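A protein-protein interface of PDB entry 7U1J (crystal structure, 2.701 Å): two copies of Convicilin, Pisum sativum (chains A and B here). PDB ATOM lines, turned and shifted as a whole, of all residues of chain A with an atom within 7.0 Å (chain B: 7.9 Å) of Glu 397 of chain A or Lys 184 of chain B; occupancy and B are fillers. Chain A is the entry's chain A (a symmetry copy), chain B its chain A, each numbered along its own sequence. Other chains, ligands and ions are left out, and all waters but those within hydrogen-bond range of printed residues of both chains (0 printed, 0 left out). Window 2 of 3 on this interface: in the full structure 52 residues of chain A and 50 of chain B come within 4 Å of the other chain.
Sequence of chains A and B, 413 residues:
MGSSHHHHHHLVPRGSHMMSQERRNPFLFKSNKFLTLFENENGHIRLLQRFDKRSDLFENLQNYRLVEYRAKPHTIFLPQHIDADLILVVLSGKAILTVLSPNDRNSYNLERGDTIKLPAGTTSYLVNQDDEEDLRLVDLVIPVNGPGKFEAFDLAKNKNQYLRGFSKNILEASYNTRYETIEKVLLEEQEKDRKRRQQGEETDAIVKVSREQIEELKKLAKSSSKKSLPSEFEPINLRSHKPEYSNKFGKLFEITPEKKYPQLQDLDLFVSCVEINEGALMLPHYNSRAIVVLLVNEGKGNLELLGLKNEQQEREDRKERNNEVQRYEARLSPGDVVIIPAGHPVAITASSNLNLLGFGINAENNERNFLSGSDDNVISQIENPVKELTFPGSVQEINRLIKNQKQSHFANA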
ATOM      1  N   PHE A 391     -23.378  -6.856  -3.589  1.00  0.00           N
ATOM      2  CA  PHE A 391     -23.137  -5.569  -2.895  1.00  0.00           C
ATOM      3  C   PHE A 391     -21.671  -5.420  -2.485  1.00  0.00           C
ATOM      4  O   PHE A 391     -20.929  -6.391  -2.281  1.00  0.00           O
ATOM      5  CB  PHE A 391     -24.031  -5.446  -1.673  1.00  0.00           C
ATOM      6  CG  PHE A 391     -25.482  -5.743  -1.914  1.00  0.00           C
ATOM      7  CD1 PHE A 391     -26.285  -4.821  -2.548  1.00  0.00           C
ATOM      8  CD2 PHE A 391     -26.045  -6.916  -1.457  1.00  0.00           C
ATOM      9  CE1 PHE A 391     -27.624  -5.082  -2.750  1.00  0.00           C
ATOM     10  CE2 PHE A 391     -27.389  -7.180  -1.664  1.00  0.00           C
ATOM     11  CZ  PHE A 391     -28.171  -6.256  -2.308  1.00  0.00           C
ATOM     12  N   PRO A 392     -21.204  -4.160  -2.359  1.00  0.00           N
ATOM     13  CA  PRO A 392     -19.784  -3.885  -2.175  1.00  0.00           C
ATOM     14  C   PRO A 392     -19.285  -4.350  -0.805  1.00  0.00           C
ATOM     15  O   PRO A 392     -18.132  -4.658  -0.682  1.00  0.00           O
ATOM     16  CB  PRO A 392     -19.670  -2.369  -2.339  1.00  0.00           C
ATOM     17  CG  PRO A 392     -21.035  -1.862  -2.032  1.00  0.00           C
ATOM     18  CD  PRO A 392     -22.011  -2.939  -2.429  1.00  0.00           C
ATOM     19  N   GLY A 393     -20.175  -4.400   0.177  1.00  0.00           N
ATOM     20  CA  GLY A 393     -19.808  -4.763   1.548  1.00  0.00           C
ATOM     21  C   GLY A 393     -19.602  -6.258   1.688  1.00  0.00           C
ATOM     22  O   GLY A 393     -19.943  -7.002   0.748  1.00  0.00           O
ATOM     23  N   SER A 394     -19.076  -6.675   2.839  1.00  0.00           N
ATOM     24  CA  SER A 394     -18.886  -8.089   3.235  1.00  0.00           C
ATOM     25  C   SER A 394     -20.252  -8.676   3.554  1.00  0.00           C
ATOM     26  O   SER A 394     -21.153  -7.920   3.793  1.00  0.00           O
ATOM     27  CB  SER A 394     -17.970  -8.193   4.420  1.00  0.00           C
ATOM     28  OG  SER A 394     -18.589  -7.661   5.590  1.00  0.00           O
ATOM     29  N   VAL A 395     -20.358  -9.987   3.623  1.00  0.00           N
ATOM     30  CA  VAL A 395     -21.585 -10.691   4.084  1.00  0.00           C
ATOM     31  C   VAL A 395     -22.015 -10.106   5.432  1.00  0.00           C
ATOM     32  O   VAL A 395     -23.250  -9.888   5.638  1.00  0.00           O
ATOM     33  CB  VAL A 395     -21.299 -12.197   4.197  1.00  0.00           C
ATOM     34  CG1 VAL A 395     -22.533 -12.996   4.563  1.00  0.00           C
ATOM     35  CG2 VAL A 395     -20.673 -12.729   2.919  1.00  0.00           C
ATOM     36  N   GLN A 396     -21.046  -9.882   6.327  1.00  0.00           N
ATOM     37  CA  GLN A 396     -21.311  -9.580   7.756  1.00  0.00           C
ATOM     38  C   GLN A 396     -21.829  -8.141   7.832  1.00  0.00           C
ATOM     39  O   GLN A 396     -22.861  -7.946   8.523  1.00  0.00           O
ATOM     40  CB  GLN A 396     -20.065  -9.856   8.596  1.00  0.00           C
ATOM     41  CG  GLN A 396     -19.496 -11.262   8.392  1.00  0.00           C
ATOM     42  CD  GLN A 396     -18.248 -11.311   7.534  1.00  0.00           C
ATOM     43  OE1 GLN A 396     -18.273 -11.105   6.326  1.00  0.00           O
ATOM     44  NE2 GLN A 396     -17.123 -11.592   8.167  1.00  0.00           N
ATOM     45  N   GLU A 397     -21.163  -7.202   7.131  1.00  0.00           N
ATOM     46  CA  GLU A 397     -21.606  -5.784   6.994  1.00  0.00           C
ATOM     47  C   GLU A 397     -23.014  -5.718   6.355  1.00  0.00           C
ATOM     48  O   GLU A 397     -23.797  -4.844   6.777  1.00  0.00           O
ATOM     49  CB  GLU A 397     -20.642  -4.933   6.150  1.00  0.00           C
ATOM     50  CG  GLU A 397     -19.202  -4.927   6.609  1.00  0.00           C
ATOM     51  CD  GLU A 397     -18.274  -4.069   5.766  1.00  0.00           C
ATOM     52  OE1 GLU A 397     -18.218  -4.265   4.548  1.00  0.00           O
ATOM     53  OE2 GLU A 397     -17.575  -3.224   6.337  1.00  0.00           O
ATOM     54  N   ILE A 398     -23.343  -6.588   5.391  1.00  0.00           N
ATOM     55  CA  ILE A 398     -24.643  -6.546   4.650  1.00  0.00           C
ATOM     56  C   ILE A 398     -25.767  -7.090   5.542  1.00  0.00           C
ATOM     57  O   ILE A 398     -26.792  -6.392   5.705  1.00  0.00           O
ATOM     58  CB  ILE A 398     -24.553  -7.310   3.320  1.00  0.00           C
ATOM     59  CG1 ILE A 398     -23.640  -6.604   2.323  1.00  0.00           C
ATOM     60  CG2 ILE A 398     -25.923  -7.531   2.719  1.00  0.00           C
ATOM     61  CD1 ILE A 398     -23.082  -7.544   1.282  1.00  0.00           C
ATOM     62  N   ASN A 399     -25.586  -8.287   6.094  1.00  0.00           N
ATOM     63  CA  ASN A 399     -26.574  -8.920   7.003  1.00  0.00           C
ATOM     64  C   ASN A 399     -26.814  -8.038   8.229  1.00  0.00           C
ATOM     65  O   ASN A 399     -27.994  -7.951   8.664  1.00  0.00           O
ATOM     66  CB  ASN A 399     -26.163 -10.350   7.305  1.00  0.00           C
ATOM     67  CG  ASN A 399     -26.323 -11.174   6.046  1.00  0.00           C
ATOM     68  OD1 ASN A 399     -27.191 -10.878   5.218  1.00  0.00           O
ATOM     69  ND2 ASN A 399     -25.470 -12.165   5.858  1.00  0.00           N
ATOM     70  N   ARG A 400     -25.779  -7.352   8.717  1.00  0.00           N
ATOM     71  CA  ARG A 400     -25.890  -6.448   9.884  1.00  0.00           C
ATOM     72  C   ARG A 400     -26.705  -5.212   9.491  1.00  0.00           C
ATOM     73  O   ARG A 400     -27.576  -4.783  10.313  1.00  0.00           O
ATOM     74  CB  ARG A 400     -24.509  -6.042  10.415  1.00  0.00           C
ATOM     75  CG  ARG A 400     -24.588  -5.123  11.628  1.00  0.00           C
ATOM     76  CD  ARG A 400     -23.243  -4.811  12.270  1.00  0.00           C
ATOM     77  NE  ARG A 400     -22.383  -3.870  11.532  1.00  0.00           N
ATOM     78  CZ  ARG A 400     -21.186  -4.151  10.993  1.00  0.00           C
ATOM     79  NH1 ARG A 400     -20.646  -5.368  11.054  1.00  0.00           N
ATOM     80  NH2 ARG A 400     -20.531  -3.185  10.367  1.00  0.00           N
ATOM     81  N   LEU A 401     -26.405  -4.630   8.320  1.00  0.00           N
ATOM     82  CA  LEU A 401     -27.086  -3.396   7.857  1.00  0.00           C
ATOM     83  C   LEU A 401     -28.573  -3.687   7.731  1.00  0.00           C
ATOM     84  O   LEU A 401     -29.397  -2.831   8.110  1.00  0.00           O
ATOM     85  CB  LEU A 401     -26.509  -2.907   6.531  1.00  0.00           C
ATOM     86  CG  LEU A 401     -27.044  -1.551   6.083  1.00  0.00           C
ATOM     87  CD1 LEU A 401     -26.026  -0.819   5.252  1.00  0.00           C
ATOM     88  CD2 LEU A 401     -28.348  -1.705   5.316  1.00  0.00           C
ATOM     89  N   ILE A 402     -28.896  -4.885   7.264  1.00  0.00           N
ATOM     90  CA  ILE A 402     -30.298  -5.287   6.950  1.00  0.00           C
ATOM     91  C   ILE A 402     -31.056  -5.565   8.242  1.00  0.00           C
ATOM     92  O   ILE A 402     -32.301  -5.650   8.187  1.00  0.00           O
ATOM     93  CB  ILE A 402     -30.260  -6.484   5.990  1.00  0.00           C
ATOM     94  CG1 ILE A 402     -30.023  -5.979   4.569  1.00  0.00           C
ATOM     95  CG2 ILE A 402     -31.505  -7.337   6.070  1.00  0.00           C
ATOM     96  CD1 ILE A 402     -29.476  -7.042   3.697  1.00  0.00           C
ATOM     97  N   ASN A 404     -30.614  -3.631  10.954  1.00  0.00           N
ATOM     98  CA  ASN A 404     -30.764  -2.313  11.626  1.00  0.00           C
ATOM     99  C   ASN A 404     -32.207  -1.810  11.557  1.00  0.00           C
ATOM    100  O   ASN A 404     -32.598  -1.007  12.444  1.00  0.00           O
ATOM    101  CB  ASN A 404     -29.843  -1.257  11.024  1.00  0.00           C
ATOM    102  CG  ASN A 404     -28.385  -1.513  11.309  1.00  0.00           C
ATOM    103  OD1 ASN A 404     -28.027  -2.354  12.141  1.00  0.00           O
ATOM    104  ND2 ASN A 404     -27.541  -0.752  10.642  1.00  0.00           N
ATOM    105  N   THR B 177     -29.989   3.176   8.928  1.00  0.00           N
ATOM    106  CA  THR B 177     -28.518   3.203   8.838  1.00  0.00           C
ATOM    107  C   THR B 177     -28.143   4.564   8.264  1.00  0.00           C
ATOM    108  O   THR B 177     -28.997   5.168   7.545  1.00  0.00           O
ATOM    109  CB  THR B 177     -28.050   2.035   7.980  1.00  0.00           C
ATOM    110  OG1 THR B 177     -28.671   0.931   8.638  1.00  0.00           O
ATOM    111  CG2 THR B 177     -26.545   1.939   7.886  1.00  0.00           C
ATOM    112  N   ARG B 178     -26.987   5.076   8.655  1.00  0.00           N
ATOM    113  CA  ARG B 178     -26.493   6.372   8.164  1.00  0.00           C
ATOM    114  C   ARG B 178     -26.250   6.146   6.676  1.00  0.00           C
ATOM    115  O   ARG B 178     -25.883   4.996   6.306  1.00  0.00           O
ATOM    116  CB  ARG B 178     -25.274   6.752   9.000  1.00  0.00           C
ATOM    117  CG  ARG B 178     -24.691   8.128   8.722  1.00  0.00           C
ATOM    118  CD  ARG B 178     -23.618   8.409   9.753  1.00  0.00           C
ATOM    119  NE  ARG B 178     -22.360   8.864   9.177  1.00  0.00           N
ATOM    120  CZ  ARG B 178     -22.151  10.111   8.815  1.00  0.00           C
ATOM    121  NH1 ARG B 178     -23.130  10.991   8.951  1.00  0.00           N
ATOM    122  NH2 ARG B 178     -20.991  10.466   8.299  1.00  0.00           N
ATOM    123  N   TYR B 179     -26.572   7.137   5.844  1.00  0.00           N
ATOM    124  CA  TYR B 179     -26.413   7.046   4.374  1.00  0.00           C
ATOM    125  C   TYR B 179     -24.991   6.539   4.074  1.00  0.00           C
ATOM    126  O   TYR B 179     -24.800   5.621   3.240  1.00  0.00           O
ATOM    127  CB  TYR B 179     -26.734   8.380   3.690  1.00  0.00           C
ATOM    128  CG  TYR B 179     -26.503   8.291   2.206  1.00  0.00           C
ATOM    129  CD1 TYR B 179     -27.370   7.566   1.404  1.00  0.00           C
ATOM    130  CD2 TYR B 179     -25.345   8.797   1.629  1.00  0.00           C
ATOM    131  CE1 TYR B 179     -27.146   7.420   0.045  1.00  0.00           C
ATOM    132  CE2 TYR B 179     -25.089   8.633   0.279  1.00  0.00           C
ATOM    133  CZ  TYR B 179     -25.995   7.941  -0.513  1.00  0.00           C
ATOM    134  OH  TYR B 179     -25.760   7.773  -1.841  1.00  0.00           O
ATOM    135  N   GLU B 180     -23.980   7.100   4.737  1.00  0.00           N
ATOM    136  CA  GLU B 180     -22.574   6.789   4.375  1.00  0.00           C
ATOM    137  C   GLU B 180     -22.388   5.273   4.411  1.00  0.00           C
ATOM    138  O   GLU B 180     -21.662   4.741   3.556  1.00  0.00           O
ATOM    139  CB  GLU B 180     -21.575   7.511   5.281  1.00  0.00           C
ATOM    140  CG  GLU B 180     -21.281   8.941   4.857  1.00  0.00           C
ATOM    141  CD  GLU B 180     -22.318   9.994   5.233  1.00  0.00           C
ATOM    142  OE1 GLU B 180     -22.063  11.208   4.898  1.00  0.00           O
ATOM    143  OE2 GLU B 180     -23.384   9.618   5.835  1.00  0.00           O
ATOM    144  N   THR B 181     -23.000   4.596   5.374  1.00  0.00           N
ATOM    145  CA  THR B 181     -22.841   3.133   5.500  1.00  0.00           C
ATOM    146  C   THR B 181     -23.638   2.426   4.395  1.00  0.00           C
ATOM    147  O   THR B 181     -23.091   1.468   3.833  1.00  0.00           O
ATOM    148  CB  THR B 181     -23.199   2.669   6.915  1.00  0.00           C
ATOM    149  OG1 THR B 181     -22.221   3.334   7.710  1.00  0.00           O
ATOM    150  CG2 THR B 181     -23.144   1.166   7.118  1.00  0.00           C
ATOM    151  N   ILE B 182     -24.887   2.836   4.140  1.00  0.00           N
ATOM    152  CA  ILE B 182     -25.728   2.323   3.019  1.00  0.00           C
ATOM    153  C   ILE B 182     -24.882   2.402   1.741  1.00  0.00           C
ATOM    154  O   ILE B 182     -24.743   1.373   1.051  1.00  0.00           O
ATOM    155  CB  ILE B 182     -27.032   3.133   2.906  1.00  0.00           C
ATOM    156  CG1 ILE B 182     -27.972   2.908   4.096  1.00  0.00           C
ATOM    157  CG2 ILE B 182     -27.697   2.838   1.581  1.00  0.00           C
ATOM    158  CD1 ILE B 182     -28.978   4.007   4.314  1.00  0.00           C
ATOM    159  N   GLU B 183     -24.249   3.557   1.496  1.00  0.00           N
ATOM    160  CA  GLU B 183     -23.371   3.804   0.321  1.00  0.00           C
ATOM    161  C   GLU B 183     -22.219   2.787   0.280  1.00  0.00           C
ATOM    162  O   GLU B 183     -21.855   2.365  -0.805  1.00  0.00           O
ATOM    163  CB  GLU B 183     -22.875   5.250   0.366  1.00  0.00           C
ATOM    164  CG  GLU B 183     -22.112   5.717  -0.862  1.00  0.00           C
ATOM    165  CD  GLU B 183     -21.842   7.211  -0.788  1.00  0.00           C
ATOM    166  OE1 GLU B 183     -21.566   7.692   0.333  1.00  0.00           O
ATOM    167  OE2 GLU B 183     -21.963   7.905  -1.818  1.00  0.00           O
ATOM    168  N   LYS B 184     -21.632   2.443   1.408  1.00  0.00           N
ATOM    169  CA  LYS B 184     -20.364   1.678   1.470  1.00  0.00           C
ATOM    170  C   LYS B 184     -20.695   0.184   1.394  1.00  0.00           C
ATOM    171  O   LYS B 184     -19.901  -0.574   0.869  1.00  0.00           O
ATOM    172  CB  LYS B 184     -19.577   2.093   2.726  1.00  0.00           C
ATOM    173  CG  LYS B 184     -18.740   0.997   3.386  1.00  0.00           C
ATOM    174  CD  LYS B 184     -17.638   1.489   4.326  1.00  0.00           C
ATOM    175  CE  LYS B 184     -16.393   0.624   4.277  1.00  0.00           C
ATOM    176  NZ  LYS B 184     -16.581  -0.640   5.033  1.00  0.00           N
ATOM    177  N   VAL B 185     -21.857  -0.220   1.867  1.00  0.00           N
ATOM    178  CA  VAL B 185     -22.212  -1.649   2.067  1.00  0.00           C
ATOM    179  C   VAL B 185     -23.103  -2.112   0.925  1.00  0.00           C
ATOM    180  O   VAL B 185     -22.858  -3.223   0.452  1.00  0.00           O
ATOM    181  CB  VAL B 185     -22.900  -1.826   3.426  1.00  0.00           C
ATOM    182  CG1 VAL B 185     -23.501  -3.210   3.594  1.00  0.00           C
ATOM    183  CG2 VAL B 185     -21.925  -1.499   4.558  1.00  0.00           C
ATOM    184  N   LEU B 186     -24.076  -1.303   0.498  1.00  0.00           N
ATOM    185  CA  LEU B 186     -25.105  -1.706  -0.512  1.00  0.00           C
ATOM    186  C   LEU B 186     -24.869  -1.071  -1.899  1.00  0.00           C
ATOM    187  O   LEU B 186     -25.166  -1.768  -2.876  1.00  0.00           O
ATOM    188  CB  LEU B 186     -26.509  -1.360   0.004  1.00  0.00           C
ATOM    189  CG  LEU B 186     -27.034  -2.183   1.182  1.00  0.00           C
ATOM    190  CD1 LEU B 186     -28.524  -1.927   1.391  1.00  0.00           C
ATOM    191  CD2 LEU B 186     -26.771  -3.657   0.961  1.00  0.00           C
ATOM    192  N   LEU B 187     -24.369   0.171  -2.001  1.00  0.00           N
ATOM    193  CA  LEU B 187     -24.517   1.017  -3.213  1.00  0.00           C
ATOM    194  C   LEU B 187     -23.199   1.168  -3.980  1.00  0.00           C
ATOM    195  O   LEU B 187     -23.203   0.836  -5.186  1.00  0.00           O
ATOM    196  CB  LEU B 187     -25.077   2.383  -2.828  1.00  0.00           C
ATOM    197  CG  LEU B 187     -26.336   2.369  -1.966  1.00  0.00           C
ATOM    198  CD1 LEU B 187     -26.954   3.747  -1.892  1.00  0.00           C
ATOM    199  CD2 LEU B 187     -27.376   1.376  -2.460  1.00  0.00           C
ATOM    200  N   GLU B 188     -22.132   1.708  -3.376  1.00  0.00           N
ATOM    201  CA  GLU B 188     -20.825   1.855  -4.082  1.00  0.00           C
ATOM    202  C   GLU B 188     -19.688   2.092  -3.081  1.00  0.00           C
ATOM    203  O   GLU B 188     -18.630   1.424  -3.260  1.00  0.00           O
ATOM    204  CB  GLU B 188     -20.898   2.982  -5.115  1.00  0.00           C
ATOM    205  CG  GLU B 188     -20.193   2.645  -6.418  1.00  0.00           C
ATOM    206  CD  GLU B 188     -20.081   3.794  -7.414  1.00  0.00           C
ATOM    207  OE1 GLU B 188     -20.296   4.973  -7.017  1.00  0.00           O
ATOM    208  OE2 GLU B 188     -19.771   3.516  -8.596  1.00  0.00           O
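Among the printed residues, merely in contact across the chains: Phe 391 of chain A with Val 185 of chain B (3.3 Å), Phe 391 of chain A with Leu 186 of chain B (3.3 Å), Pro 392 of chain A with Lys 184 of chain B (3.4 Å), Pro 392 of chain A with Leu 186 of chain B (3.4 Å), Pro 392 of chain A with Leu 187 of chain B (3.9 Å), Pro 392 of chain A with Glu 188 of chain B (3.97 Å), Gly 393 of chain A with Lys 184 of chain B (3.9 Å), Glu 397 of chain A with Val 185 of chain B (3.6 Å), Ile 398 of chain A with Val 185 of chain B (3.6 Å), Leu 401 of chain A with Thr 177 of chain B (3.8 Å), Leu 401 of chain A with Thr 181 of chain B (3.97 Å), Leu 401 of chain A with Ile 182 of chain B (3.9 Å), Leu 401 of chain A with Val 185 of chain B (3.8 Å) and Leu 401 of chain A with Leu 186 of chain B (3.9 Å).
ND2 of Asn 404 of chain A lies within hydrogen-bond range of OG1 of Thr 177 of chain B. OE2 of Glu 397 of chain A lies within salt-bridge range of NZ of Lys 184 of chain B, at 3.1 Å. O of Val 185 of chain B is in hydrogen-bond range of N of Gly 393 of chain A. The backbone nitrogen of Pro 392 of chain A sits close to the backbone carbonyl oxygen of Val 185 of chain B, 3.4 Å away.
No position is printed for both chains.
The backbone NH of Leu 187 of chain B is in hydrogen-bond range of the backbone carbonyl oxygen of Ile 182 of chain B (3.3 Å). The backbone carbonyl oxygen (O) of Glu 183 of chain B lies within hydrogen-bond range of the backbone NH (N) of Glu 188 of chain B (2.7 Å). The backbone NH (N) of Glu 397 of chain A sits close to the side-chain hydroxyl (OG) of Ser 394 of chain A, at 3.0 Å. The backbone carbonyl oxygen of Arg 400 of chain A lies close to the side-chain amide oxygen of Asn 404 of chain A (3.1 Å).
Glu 397 of chain A touches two residues of chain B. Of the printed residues of chain B, Leu 401 of chain A touches Thr 177, Thr 181, Ile 182, Val 185 and Leu 186. Printed residues of chain B within 4 Å of Asn 404 of chain A: Thr 177. Printed residues of chain A within 4 Å of Thr 177 of chain B: Leu 401 and Asn 404. Of chain A, only Pro 392, Gly 393 and Glu 397 come within 4 Å of Lys 184 of chain B. Printed residues of chain A within 4 Å of Val 185 of chain B: Phe 391 (3.3 Å), Pro 392 (3.0 Å), Gly 393 (2.9 Å), Glu 397 (3.6 Å), Ile 398 (3.6 Å) and Leu 401 (3.8 Å). The nearest residue of chain B that does not touch Glu 397 of chain A is Thr 181 of chain B (6.1 Å). The nearest printed residue of chain B that does not touch Gly 393 of chain A is Leu 186 of chain B (5.0 Å).
Of the 12 printed residues of chain B, 8 touch a printed residue of chain A. Along chain B the printed residues that touch a printed residue of chain A span positions 177 to 188. Of the 13 printed residues of chain A, 7 touch a printed residue of chain B. Hydrophobic or aromatic side chains of chain A within 4 Å of the printed part of chain B: Phe 391, Pro 392, Ile 398 and Leu 401. Among the printed residues, 18 pairs touch across the chains. Among the printed residues, Asp or Glu carboxylates within 4 Å of a Lys or Arg side-chain nitrogen of the other chain: Glu 397 of chain A with Lys 184 of chain B (3.1 Å).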
